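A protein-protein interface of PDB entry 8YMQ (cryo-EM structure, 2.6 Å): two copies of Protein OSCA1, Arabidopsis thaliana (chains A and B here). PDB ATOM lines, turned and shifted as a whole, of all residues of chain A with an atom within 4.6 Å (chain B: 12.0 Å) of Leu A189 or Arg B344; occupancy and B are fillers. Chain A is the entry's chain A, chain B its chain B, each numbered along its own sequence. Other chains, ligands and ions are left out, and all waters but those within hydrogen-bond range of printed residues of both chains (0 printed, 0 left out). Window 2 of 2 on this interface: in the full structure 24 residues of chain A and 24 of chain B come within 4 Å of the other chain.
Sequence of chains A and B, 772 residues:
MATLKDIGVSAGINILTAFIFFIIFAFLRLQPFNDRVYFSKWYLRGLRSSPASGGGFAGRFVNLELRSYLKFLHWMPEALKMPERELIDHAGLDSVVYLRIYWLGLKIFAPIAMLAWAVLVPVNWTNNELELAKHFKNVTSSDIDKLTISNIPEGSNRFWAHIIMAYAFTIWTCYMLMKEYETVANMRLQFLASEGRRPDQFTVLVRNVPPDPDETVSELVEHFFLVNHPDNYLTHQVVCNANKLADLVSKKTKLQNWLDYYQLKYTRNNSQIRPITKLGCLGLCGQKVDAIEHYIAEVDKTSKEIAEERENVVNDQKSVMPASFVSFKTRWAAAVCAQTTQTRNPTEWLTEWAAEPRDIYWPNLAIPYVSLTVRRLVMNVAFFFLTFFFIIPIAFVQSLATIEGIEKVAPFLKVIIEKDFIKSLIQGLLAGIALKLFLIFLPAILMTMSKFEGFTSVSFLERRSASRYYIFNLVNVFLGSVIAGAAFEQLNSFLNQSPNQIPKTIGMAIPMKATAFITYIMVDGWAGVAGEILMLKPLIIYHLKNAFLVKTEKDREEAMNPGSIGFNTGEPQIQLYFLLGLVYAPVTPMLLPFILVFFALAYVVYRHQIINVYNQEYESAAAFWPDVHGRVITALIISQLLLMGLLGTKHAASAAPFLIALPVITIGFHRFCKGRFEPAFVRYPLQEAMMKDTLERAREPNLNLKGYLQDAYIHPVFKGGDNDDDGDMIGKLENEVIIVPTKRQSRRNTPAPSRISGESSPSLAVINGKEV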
ATOM      1  N   ALA A 185       8.291   4.735 -26.862  1.00  0.00           N
ATOM      2  CA  ALA A 185       7.483   3.938 -25.953  1.00  0.00           C
ATOM      3  C   ALA A 185       7.079   4.752 -24.767  1.00  0.00           C
ATOM      4  O   ALA A 185       5.933   4.727 -24.375  1.00  0.00           O
ATOM      5  CB  ALA A 185       8.246   2.716 -25.500  1.00  0.00           C
ATOM      6  N   ASN A 186       8.013   5.494 -24.199  1.00  0.00           N
ATOM      7  CA  ASN A 186       7.728   6.323 -23.051  1.00  0.00           C
ATOM      8  C   ASN A 186       6.804   7.457 -23.400  1.00  0.00           C
ATOM      9  O   ASN A 186       6.005   7.869 -22.579  1.00  0.00           O
ATOM     10  CB  ASN A 186       9.021   6.874 -22.475  1.00  0.00           C
ATOM     11  CG  ASN A 186       9.912   5.798 -21.905  1.00  0.00           C
ATOM     12  OD1 ASN A 186       9.438   4.769 -21.433  1.00  0.00           O
ATOM     13  ND2 ASN A 186      11.213   6.031 -21.949  1.00  0.00           N
ATOM     14  N   MET A 187       6.900   7.968 -24.615  1.00  0.00           N
ATOM     15  CA  MET A 187       6.023   9.027 -25.062  1.00  0.00           C
ATOM     16  C   MET A 187       4.618   8.516 -25.210  1.00  0.00           C
ATOM     17  O   MET A 187       3.685   9.201 -24.849  1.00  0.00           O
ATOM     18  CB  MET A 187       6.506   9.564 -26.396  1.00  0.00           C
ATOM     19  CG  MET A 187       7.162  10.929 -26.328  1.00  0.00           C
ATOM     20  SD  MET A 187       7.647  11.546 -27.951  1.00  0.00           S
ATOM     21  CE  MET A 187       9.057  10.510 -28.283  1.00  0.00           C
ATOM     22  N   ARG A 188       4.461   7.309 -25.734  1.00  0.00           N
ATOM     23  CA  ARG A 188       3.147   6.721 -25.931  1.00  0.00           C
ATOM     24  C   ARG A 188       2.504   6.415 -24.617  1.00  0.00           C
ATOM     25  O   ARG A 188       1.314   6.605 -24.460  1.00  0.00           O
ATOM     26  CB  ARG A 188       3.249   5.485 -26.824  1.00  0.00           C
ATOM     27  CG  ARG A 188       2.531   4.235 -26.359  1.00  0.00           C
ATOM     28  CD  ARG A 188       2.187   3.370 -27.546  1.00  0.00           C
ATOM     29  NE  ARG A 188       1.110   2.438 -27.267  1.00  0.00           N
ATOM     30  CZ  ARG A 188       0.030   2.304 -28.023  1.00  0.00           C
ATOM     31  NH1 ARG A 188      -0.119   3.050 -29.098  1.00  0.00           N
ATOM     32  NH2 ARG A 188      -0.903   1.427 -27.698  1.00  0.00           N
ATOM     33  N   LEU A 189       3.297   6.003 -23.644  1.00  0.00           N
ATOM     34  CA  LEU A 189       2.769   5.660 -22.348  1.00  0.00           C
ATOM     35  C   LEU A 189       2.338   6.892 -21.600  1.00  0.00           C
ATOM     36  O   LEU A 189       1.308   6.878 -20.949  1.00  0.00           O
ATOM     37  CB  LEU A 189       3.797   4.859 -21.574  1.00  0.00           C
ATOM     38  CG  LEU A 189       3.930   3.405 -22.023  1.00  0.00           C
ATOM     39  CD1 LEU A 189       5.171   2.774 -21.416  1.00  0.00           C
ATOM     40  CD2 LEU A 189       2.684   2.601 -21.693  1.00  0.00           C
ATOM     41  N   GLN A 190       3.095   7.972 -21.711  1.00  0.00           N
ATOM     42  CA  GLN A 190       2.721   9.228 -21.083  1.00  0.00           C
ATOM     43  C   GLN A 190       1.491   9.819 -21.741  1.00  0.00           C
ATOM     44  O   GLN A 190       0.617  10.351 -21.066  1.00  0.00           O
ATOM     45  CB  GLN A 190       3.911  10.191 -21.118  1.00  0.00           C
ATOM     46  CG  GLN A 190       3.664  11.593 -21.660  1.00  0.00           C
ATOM     47  CD  GLN A 190       4.531  11.921 -22.864  1.00  0.00           C
ATOM     48  OE1 GLN A 190       5.758  11.978 -22.760  1.00  0.00           O
ATOM     49  NE2 GLN A 190       3.898  12.138 -24.015  1.00  0.00           N
ATOM     50  N   PHE A 191       1.384   9.684 -23.050  1.00  0.00           N
ATOM     51  CA  PHE A 191       0.261  10.221 -23.775  1.00  0.00           C
ATOM     52  C   PHE A 191      -0.981   9.472 -23.414  1.00  0.00           C
ATOM     53  O   PHE A 191      -2.023  10.069 -23.228  1.00  0.00           O
ATOM     54  CB  PHE A 191       0.524  10.073 -25.264  1.00  0.00           C
ATOM     55  CG  PHE A 191      -0.497  10.720 -26.135  1.00  0.00           C
ATOM     56  CD1 PHE A 191      -0.503  12.085 -26.313  1.00  0.00           C
ATOM     57  CD2 PHE A 191      -1.440   9.961 -26.790  1.00  0.00           C
ATOM     58  CE1 PHE A 191      -1.439  12.687 -27.121  1.00  0.00           C
ATOM     59  CE2 PHE A 191      -2.379  10.554 -27.591  1.00  0.00           C
ATOM     60  CZ  PHE A 191      -2.381  11.920 -27.759  1.00  0.00           C
ATOM     61  N   LEU A 192      -0.885   8.159 -23.305  1.00  0.00           N
ATOM     62  CA  LEU A 192      -2.045   7.344 -23.024  1.00  0.00           C
ATOM     63  C   LEU A 192      -2.566   7.595 -21.640  1.00  0.00           C
ATOM     64  O   LEU A 192      -3.755   7.488 -21.408  1.00  0.00           O
ATOM     65  CB  LEU A 192      -1.683   5.881 -23.176  1.00  0.00           C
ATOM     66  CG  LEU A 192      -2.210   5.104 -24.376  1.00  0.00           C
ATOM     67  CD1 LEU A 192      -2.607   6.027 -25.511  1.00  0.00           C
ATOM     68  CD2 LEU A 192      -1.175   4.093 -24.828  1.00  0.00           C
ATOM     69  N   ALA A 193      -1.688   7.949 -20.716  1.00  0.00           N
ATOM     70  CA  ALA A 193      -2.077   8.212 -19.343  1.00  0.00           C
ATOM     71  C   ALA A 193      -2.739   9.551 -19.173  1.00  0.00           C
ATOM     72  O   ALA A 193      -3.487   9.757 -18.229  1.00  0.00           O
ATOM     73  CB  ALA A 193      -0.856   8.143 -18.464  1.00  0.00           C
ATOM     74  N   ARG A 676      11.433  -5.755 -24.979  1.00  0.00           N
ATOM     75  CA  ARG A 676      11.576  -4.693 -24.017  1.00  0.00           C
ATOM     76  C   ARG A 676      10.731  -3.509 -24.366  1.00  0.00           C
ATOM     77  O   ARG A 676      10.083  -2.939 -23.501  1.00  0.00           O
ATOM     78  CB  ARG A 676      13.030  -4.248 -23.932  1.00  0.00           C
ATOM     79  CG  ARG A 676      13.669  -4.456 -22.573  1.00  0.00           C
ATOM     80  CD  ARG A 676      13.795  -3.147 -21.815  1.00  0.00           C
ATOM     81  NE  ARG A 676      12.490  -2.617 -21.432  1.00  0.00           N
ATOM     82  CZ  ARG A 676      12.287  -1.402 -20.940  1.00  0.00           C
ATOM     83  NH1 ARG A 676      13.307  -0.576 -20.761  1.00  0.00           N
ATOM     84  NH2 ARG A 676      11.061  -1.013 -20.628  1.00  0.00           N
ATOM     85  N   ALA A 680       4.953  -2.090 -25.081  1.00  0.00           N
ATOM     86  CA  ALA A 680       4.254  -0.839 -24.825  1.00  0.00           C
ATOM     87  C   ALA A 680       3.305  -0.442 -25.916  1.00  0.00           C
ATOM     88  O   ALA A 680       2.446   0.396 -25.702  1.00  0.00           O
ATOM     89  CB  ALA A 680       5.262   0.265 -24.620  1.00  0.00           C
ATOM     90  N   PRO A 685      -0.890  -2.213 -20.150  1.00  0.00           N
ATOM     91  CA  PRO A 685      -0.695  -2.696 -18.792  1.00  0.00           C
ATOM     92  C   PRO A 685      -1.900  -2.458 -17.901  1.00  0.00           C
ATOM     93  O   PRO A 685      -2.571  -1.449 -18.023  1.00  0.00           O
ATOM     94  CB  PRO A 685       0.531  -1.931 -18.317  1.00  0.00           C
ATOM     95  CG  PRO A 685       0.816  -0.886 -19.330  1.00  0.00           C
ATOM     96  CD  PRO A 685       0.209  -1.348 -20.600  1.00  0.00           C
ATOM     97  N   GLU A 688      -1.583   0.532 -15.426  1.00  0.00           N
ATOM     98  CA  GLU A 688      -1.779   1.803 -16.072  1.00  0.00           C
ATOM     99  C   GLU A 688      -3.242   2.065 -16.230  1.00  0.00           C
ATOM    100  O   GLU A 688      -3.693   3.186 -16.045  1.00  0.00           O
ATOM    101  CB  GLU A 688      -1.103   1.758 -17.433  1.00  0.00           C
ATOM    102  CG  GLU A 688       0.163   2.588 -17.548  1.00  0.00           C
ATOM    103  CD  GLU A 688       1.222   2.209 -16.531  1.00  0.00           C
ATOM    104  OE1 GLU A 688       1.782   3.124 -15.897  1.00  0.00           O
ATOM    105  OE2 GLU A 688       1.504   1.005 -16.364  1.00  0.00           O
ATOM    106  N   VAL B 206       4.218 -14.771  -9.568  1.00  0.00           N
ATOM    107  CA  VAL B 206       4.709 -13.477  -9.982  1.00  0.00           C
ATOM    108  C   VAL B 206       6.211 -13.495  -9.811  1.00  0.00           C
ATOM    109  O   VAL B 206       6.718 -13.918  -8.796  1.00  0.00           O
ATOM    110  CB  VAL B 206       3.997 -12.293  -9.287  1.00  0.00           C
ATOM    111  CG1 VAL B 206       4.152 -12.318  -7.782  1.00  0.00           C
ATOM    112  CG2 VAL B 206       4.474 -10.979  -9.857  1.00  0.00           C
ATOM    113  N   ARG B 207       6.934 -13.105 -10.842  1.00  0.00           N
ATOM    114  CA  ARG B 207       8.369 -13.129 -10.788  1.00  0.00           C
ATOM    115  C   ARG B 207       8.843 -11.725 -10.941  1.00  0.00           C
ATOM    116  O   ARG B 207       8.074 -10.868 -11.343  1.00  0.00           O
ATOM    117  CB  ARG B 207       8.925 -13.971 -11.921  1.00  0.00           C
ATOM    118  CG  ARG B 207       8.697 -15.463 -11.790  1.00  0.00           C
ATOM    119  CD  ARG B 207       9.548 -16.202 -12.808  1.00  0.00           C
ATOM    120  NE  ARG B 207      10.270 -17.341 -12.245  1.00  0.00           N
ATOM    121  CZ  ARG B 207      11.444 -17.267 -11.621  1.00  0.00           C
ATOM    122  NH1 ARG B 207      12.053 -16.102 -11.454  1.00  0.00           N
ATOM    123  NH2 ARG B 207      12.014 -18.367 -11.155  1.00  0.00           N
ATOM    124  N   ASN B 208      10.100 -11.476 -10.600  1.00  0.00           N
ATOM    125  CA  ASN B 208      10.691 -10.149 -10.733  1.00  0.00           C
ATOM    126  C   ASN B 208       9.899  -9.035 -10.099  1.00  0.00           C
ATOM    127  O   ASN B 208       9.535  -8.087 -10.762  1.00  0.00           O
ATOM    128  CB  ASN B 208      11.014  -9.843 -12.186  1.00  0.00           C
ATOM    129  CG  ASN B 208      12.442 -10.140 -12.529  1.00  0.00           C
ATOM    130  OD1 ASN B 208      13.238 -10.480 -11.659  1.00  0.00           O
ATOM    131  ND2 ASN B 208      12.782 -10.006 -13.798  1.00  0.00           N
ATOM    132  N   PRO B 210       9.811  -5.825  -8.313  1.00  0.00           N
ATOM    133  CA  PRO B 210      10.837  -4.794  -8.161  1.00  0.00           C
ATOM    134  C   PRO B 210      11.184  -4.484  -6.715  1.00  0.00           C
ATOM    135  O   PRO B 210      10.291  -4.319  -5.891  1.00  0.00           O
ATOM    136  CB  PRO B 210      10.207  -3.578  -8.827  1.00  0.00           C
ATOM    137  CG  PRO B 210       8.761  -3.877  -8.941  1.00  0.00           C
ATOM    138  CD  PRO B 210       8.681  -5.352  -9.116  1.00  0.00           C
ATOM    139  N   PHE B 224       0.285  -4.467  -4.557  1.00  0.00           N
ATOM    140  CA  PHE B 224       0.054  -4.501  -5.987  1.00  0.00           C
ATOM    141  C   PHE B 224      -1.214  -5.216  -6.305  1.00  0.00           C
ATOM    142  O   PHE B 224      -2.021  -4.736  -7.065  1.00  0.00           O
ATOM    143  CB  PHE B 224       1.193  -5.225  -6.685  1.00  0.00           C
ATOM    144  CG  PHE B 224       1.179  -5.108  -8.182  1.00  0.00           C
ATOM    145  CD1 PHE B 224       1.756  -4.022  -8.804  1.00  0.00           C
ATOM    146  CD2 PHE B 224       0.621  -6.102  -8.967  1.00  0.00           C
ATOM    147  CE1 PHE B 224       1.756  -3.914 -10.178  1.00  0.00           C
ATOM    148  CE2 PHE B 224       0.613  -6.000 -10.336  1.00  0.00           C
ATOM    149  CZ  PHE B 224       1.181  -4.903 -10.943  1.00  0.00           C
ATOM    150  N   ASN B 228      -4.479  -3.653  -8.081  1.00  0.00           N
ATOM    151  CA  ASN B 228      -4.576  -3.942  -9.499  1.00  0.00           C
ATOM    152  C   ASN B 228      -5.469  -5.110  -9.776  1.00  0.00           C
ATOM    153  O   ASN B 228      -5.965  -5.240 -10.883  1.00  0.00           O
ATOM    154  CB  ASN B 228      -3.195  -4.120 -10.102  1.00  0.00           C
ATOM    155  CG  ASN B 228      -2.392  -2.847 -10.072  1.00  0.00           C
ATOM    156  OD1 ASN B 228      -1.339  -2.778  -9.455  1.00  0.00           O
ATOM    157  ND2 ASN B 228      -2.903  -1.817 -10.723  1.00  0.00           N
ATOM    158  N   HIS B 229      -5.683  -5.968  -8.794  1.00  0.00           N
ATOM    159  CA  HIS B 229      -6.631  -7.059  -8.939  1.00  0.00           C
ATOM    160  C   HIS B 229      -7.405  -6.965  -7.662  1.00  0.00           C
ATOM    161  O   HIS B 229      -7.425  -7.904  -6.886  1.00  0.00           O
ATOM    162  CB  HIS B 229      -5.912  -8.387  -9.036  1.00  0.00           C
ATOM    163  CG  HIS B 229      -5.203  -8.593 -10.335  1.00  0.00           C
ATOM    164  ND1 HIS B 229      -5.803  -9.184 -11.423  1.00  0.00           N
ATOM    165  CD2 HIS B 229      -3.947  -8.276 -10.725  1.00  0.00           C
ATOM    166  CE1 HIS B 229      -4.948  -9.226 -12.427  1.00  0.00           C
ATOM    167  NE2 HIS B 229      -3.814  -8.683 -12.029  1.00  0.00           N
ATOM    168  N   THR B 340      -2.525 -11.585 -18.667  1.00  0.00           N
ATOM    169  CA  THR B 340      -2.571 -10.142 -18.837  1.00  0.00           C
ATOM    170  C   THR B 340      -1.236  -9.503 -18.453  1.00  0.00           C
ATOM    171  O   THR B 340      -0.479 -10.079 -17.682  1.00  0.00           O
ATOM    172  CB  THR B 340      -3.796  -9.553 -18.092  1.00  0.00           C
ATOM    173  OG1 THR B 340      -4.484  -8.628 -18.940  1.00  0.00           O
ATOM    174  CG2 THR B 340      -3.428  -8.875 -16.786  1.00  0.00           C
ATOM    175  N   THR B 341      -0.907  -8.355 -19.038  1.00  0.00           N
ATOM    176  CA  THR B 341       0.313  -7.641 -18.671  1.00  0.00           C
ATOM    177  C   THR B 341      -0.006  -6.761 -17.500  1.00  0.00           C
ATOM    178  O   THR B 341      -1.040  -6.115 -17.472  1.00  0.00           O
ATOM    179  CB  THR B 341       0.899  -6.810 -19.822  1.00  0.00           C
ATOM    180  OG1 THR B 341       1.543  -5.646 -19.296  1.00  0.00           O
ATOM    181  CG2 THR B 341      -0.185  -6.393 -20.791  1.00  0.00           C
ATOM    182  N   GLN B 342       0.875  -6.726 -16.518  1.00  0.00           N
ATOM    183  CA  GLN B 342       0.583  -5.995 -15.306  1.00  0.00           C
ATOM    184  C   GLN B 342       1.165  -4.617 -15.233  1.00  0.00           C
ATOM    185  O   GLN B 342       0.528  -3.713 -14.718  1.00  0.00           O
ATOM    186  CB  GLN B 342       1.081  -6.802 -14.119  1.00  0.00           C
ATOM    187  CG  GLN B 342       0.867  -8.295 -14.243  1.00  0.00           C
ATOM    188  CD  GLN B 342      -0.546  -8.697 -13.907  1.00  0.00           C
ATOM    189  OE1 GLN B 342      -1.191  -8.081 -13.069  1.00  0.00           O
ATOM    190  NE2 GLN B 342      -1.032  -9.734 -14.559  1.00  0.00           N
ATOM    191  N   THR B 343       2.373  -4.437 -15.735  1.00  0.00           N
ATOM    192  CA  THR B 343       3.034  -3.160 -15.604  1.00  0.00           C
ATOM    193  C   THR B 343       3.661  -2.729 -16.914  1.00  0.00           C
ATOM    194  O   THR B 343       3.700  -3.501 -17.861  1.00  0.00           O
ATOM    195  CB  THR B 343       4.056  -3.214 -14.445  1.00  0.00           C
ATOM    196  OG1 THR B 343       4.745  -1.966 -14.322  1.00  0.00           O
ATOM    197  CG2 THR B 343       5.054  -4.306 -14.672  1.00  0.00           C
ATOM    198  N   ARG B 344       4.139  -1.492 -16.982  1.00  0.00           N
ATOM    199  CA  ARG B 344       4.744  -0.963 -18.191  1.00  0.00           C
ATOM    200  C   ARG B 344       6.135  -1.483 -18.420  1.00  0.00           C
ATOM    201  O   ARG B 344       6.650  -1.379 -19.523  1.00  0.00           O
ATOM    202  CB  ARG B 344       4.778   0.557 -18.132  1.00  0.00           C
ATOM    203  CG  ARG B 344       5.361   1.131 -16.858  1.00  0.00           C
ATOM    204  CD  ARG B 344       5.865   2.539 -17.101  1.00  0.00           C
ATOM    205  NE  ARG B 344       4.765   3.485 -17.243  1.00  0.00           N
ATOM    206  CZ  ARG B 344       4.847   4.631 -17.907  1.00  0.00           C
ATOM    207  NH1 ARG B 344       5.980   4.979 -18.496  1.00  0.00           N
ATOM    208  NH2 ARG B 344       3.794   5.430 -17.981  1.00  0.00           N
ATOM    209  N   ASN B 345       6.760  -2.025 -17.389  1.00  0.00           N
ATOM    210  CA  ASN B 345       8.070  -2.612 -17.544  1.00  0.00           C
ATOM    211  C   ASN B 345       7.853  -4.046 -17.899  1.00  0.00           C
ATOM    212  O   ASN B 345       7.295  -4.800 -17.119  1.00  0.00           O
ATOM    213  CB  ASN B 345       8.868  -2.489 -16.262  1.00  0.00           C
ATOM    214  CG  ASN B 345      10.329  -2.822 -16.454  1.00  0.00           C
ATOM    215  OD1 ASN B 345      10.760  -3.941 -16.199  1.00  0.00           O
ATOM    216  ND2 ASN B 345      11.099  -1.849 -16.912  1.00  0.00           N
ATOM    217  N   PRO B 346       8.309  -4.451 -19.083  1.00  0.00           N
ATOM    218  CA  PRO B 346       8.042  -5.812 -19.544  1.00  0.00           C
ATOM    219  C   PRO B 346       8.851  -6.900 -18.850  1.00  0.00           C
ATOM    220  O   PRO B 346       8.750  -8.051 -19.248  1.00  0.00           O
ATOM    221  CB  PRO B 346       8.423  -5.734 -21.012  1.00  0.00           C
ATOM    222  CG  PRO B 346       9.509  -4.722 -21.058  1.00  0.00           C
ATOM    223  CD  PRO B 346       9.150  -3.698 -20.028  1.00  0.00           C
ATOM    224  N   THR B 347       9.632  -6.554 -17.838  1.00  0.00           N
ATOM    225  CA  THR B 347      10.470  -7.514 -17.158  1.00  0.00           C
ATOM    226  C   THR B 347      10.232  -7.464 -15.673  1.00  0.00           C
ATOM    227  O   THR B 347      11.029  -7.978 -14.914  1.00  0.00           O
ATOM    228  CB  THR B 347      11.946  -7.210 -17.415  1.00  0.00           C
ATOM    229  OG1 THR B 347      12.082  -5.869 -17.896  1.00  0.00           O
ATOM    230  CG2 THR B 347      12.510  -8.170 -18.445  1.00  0.00           C
ATOM    231  N   GLU B 348       9.151  -6.831 -15.248  1.00  0.00           N
ATOM    232  CA  GLU B 348       8.813  -6.784 -13.843  1.00  0.00           C
ATOM    233  C   GLU B 348       7.409  -7.277 -13.686  1.00  0.00           C
ATOM    234  O   GLU B 348       6.663  -7.266 -14.654  1.00  0.00           O
ATOM    235  CB  GLU B 348       8.930  -5.376 -13.305  1.00  0.00           C
ATOM    236  CG  GLU B 348      10.291  -5.039 -12.737  1.00  0.00           C
ATOM    237  CD  GLU B 348      10.522  -3.548 -12.687  1.00  0.00           C
ATOM    238  OE1 GLU B 348       9.526  -2.804 -12.613  1.00  0.00           O
ATOM    239  OE2 GLU B 348      11.693  -3.121 -12.725  1.00  0.00           O
ATOM    240  N   TRP B 349       7.040  -7.719 -12.490  1.00  0.00           N
ATOM    241  CA  TRP B 349       5.713  -8.269 -12.227  1.00  0.00           C
ATOM    242  C   TRP B 349       5.288  -9.239 -13.292  1.00  0.00           C
ATOM    243  O   TRP B 349       4.250  -9.070 -13.902  1.00  0.00           O
ATOM    244  CB  TRP B 349       4.672  -7.176 -12.013  1.00  0.00           C
ATOM    245  CG  TRP B 349       4.941  -6.262 -10.872  1.00  0.00           C
ATOM    246  CD1 TRP B 349       5.407  -4.992 -10.946  1.00  0.00           C
ATOM    247  CD2 TRP B 349       4.734  -6.532  -9.482  1.00  0.00           C
ATOM    248  NE1 TRP B 349       5.508  -4.450  -9.695  1.00  0.00           N
ATOM    249  CE2 TRP B 349       5.106  -5.378  -8.776  1.00  0.00           C
ATOM    250  CE3 TRP B 349       4.269  -7.635  -8.768  1.00  0.00           C
ATOM    251  CZ2 TRP B 349       5.037  -5.299  -7.392  1.00  0.00           C
ATOM    252  CZ3 TRP B 349       4.202  -7.554  -7.401  1.00  0.00           C
ATOM    253  CH2 TRP B 349       4.582  -6.397  -6.727  1.00  0.00           C
ATOM    254  N   LEU B 350       6.080 -10.276 -13.503  1.00  0.00           N
ATOM    255  CA  LEU B 350       5.797 -11.242 -14.544  1.00  0.00           C
ATOM    256  C   LEU B 350       4.973 -12.374 -14.026  1.00  0.00           C
ATOM    257  O   LEU B 350       5.467 -13.210 -13.305  1.00  0.00           O
ATOM    258  CB  LEU B 350       7.105 -11.778 -15.102  1.00  0.00           C
ATOM    259  CG  LEU B 350       8.092 -10.744 -15.603  1.00  0.00           C
ATOM    260  CD1 LEU B 350       9.494 -11.311 -15.532  1.00  0.00           C
ATOM    261  CD2 LEU B 350       7.721 -10.398 -17.029  1.00  0.00           C
ATOM    262  N   THR B 351       3.720 -12.436 -14.431  1.00  0.00           N
ATOM    263  CA  THR B 351       2.818 -13.450 -13.920  1.00  0.00           C
ATOM    264  C   THR B 351       2.607 -14.613 -14.859  1.00  0.00           C
ATOM    265  O   THR B 351       2.435 -14.423 -16.051  1.00  0.00           O
ATOM    266  CB  THR B 351       1.464 -12.824 -13.583  1.00  0.00           C
ATOM    267  OG1 THR B 351       0.999 -12.079 -14.710  1.00  0.00           O
ATOM    268  CG2 THR B 351       1.606 -11.889 -12.408  1.00  0.00           C
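O of Thr B343 lies within hydrogen-bond range of OG1 of Thr B341, at 3.4 Å.
The side-chain hydroxyl (OG1) of Thr B347 lies within hydrogen-bond range of the side-chain amide oxygen (OD1) of Asn B345 (2.9 Å).
OD1 of Asn B345 lies within hydrogen-bond range of N of Glu B348, 3.4 Å away.
Leu A189 touches one residue of chain B.
Of the printed residues of chain A, Arg B344 touches Leu A189, Pro A685 and Glu A688.
No residue of chain B comes within 4 Å of Ala A185.
No residue of chain B comes within 4 Å of Asn A186.
No residue of chain B comes within 4 Å of Arg A188.
No residue of chain B comes within 4 Å of Leu A192.
No residue of chain B comes within 4 Å of Ala A193.
No residue of chain B comes within 4 Å of Ala A680.
Of the printed residues of chain B, Pro A685 touches Thr B341 (3.7 Å), Thr B343 (3.5 Å) and Arg B344 (3.9 Å).
Of the printed residues of chain A, Thr B343 touches Pro A685.
Printed residues of chain B within 4 Å of Glu A688: Arg B344 (3.3 Å).
Of the printed residues of chain B, Arg A676 touches Asn B345 and Pro B346.
Of the printed residues of chain A, Asn B345 touches Arg A676 (3.8 Å).
Phe A191 touches none of the printed residues of chain B.
Asn B228 touches none of the printed residues of chain A.
The nearest printed residue of chain A that does not touch Arg B344 is Asn A186 (4.5 Å).
The nearest printed residue of chain B that does not touch Glu A688 is Thr B343 (4.3 Å).
Printed residues of chain A that touch a printed residue of chain B: Leu A189, Arg A676, Pro A685 and Glu A688.
Along chain A the printed residues that touch a printed residue of chain B span positions 189 to 688.
Among the printed residues, 7 pairs touch across the chains.
Among the printed residues, Asp or Glu carboxylates within 4 Å of a Lys or Arg side-chain nitrogen of the other chain: Glu A688 with Arg B344 (3.3 Å).
No position is printed for both chains.
Among the printed residues, merely in contact across the chains: Leu A189 with Arg B344 (3.6 Å), Arg A676 with Asn B345 (3.8 Å), Arg A676 with Pro B346 (3.1 Å), Pro A685 with Thr B341 (3.7 Å), Pro A685 with Thr B343 (3.5 Å) and Pro A685 with Arg B344 (3.9 Å).
NE of Arg B344 lies within salt-bridge range of OE1 of Glu A688, 3.3 Å away.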
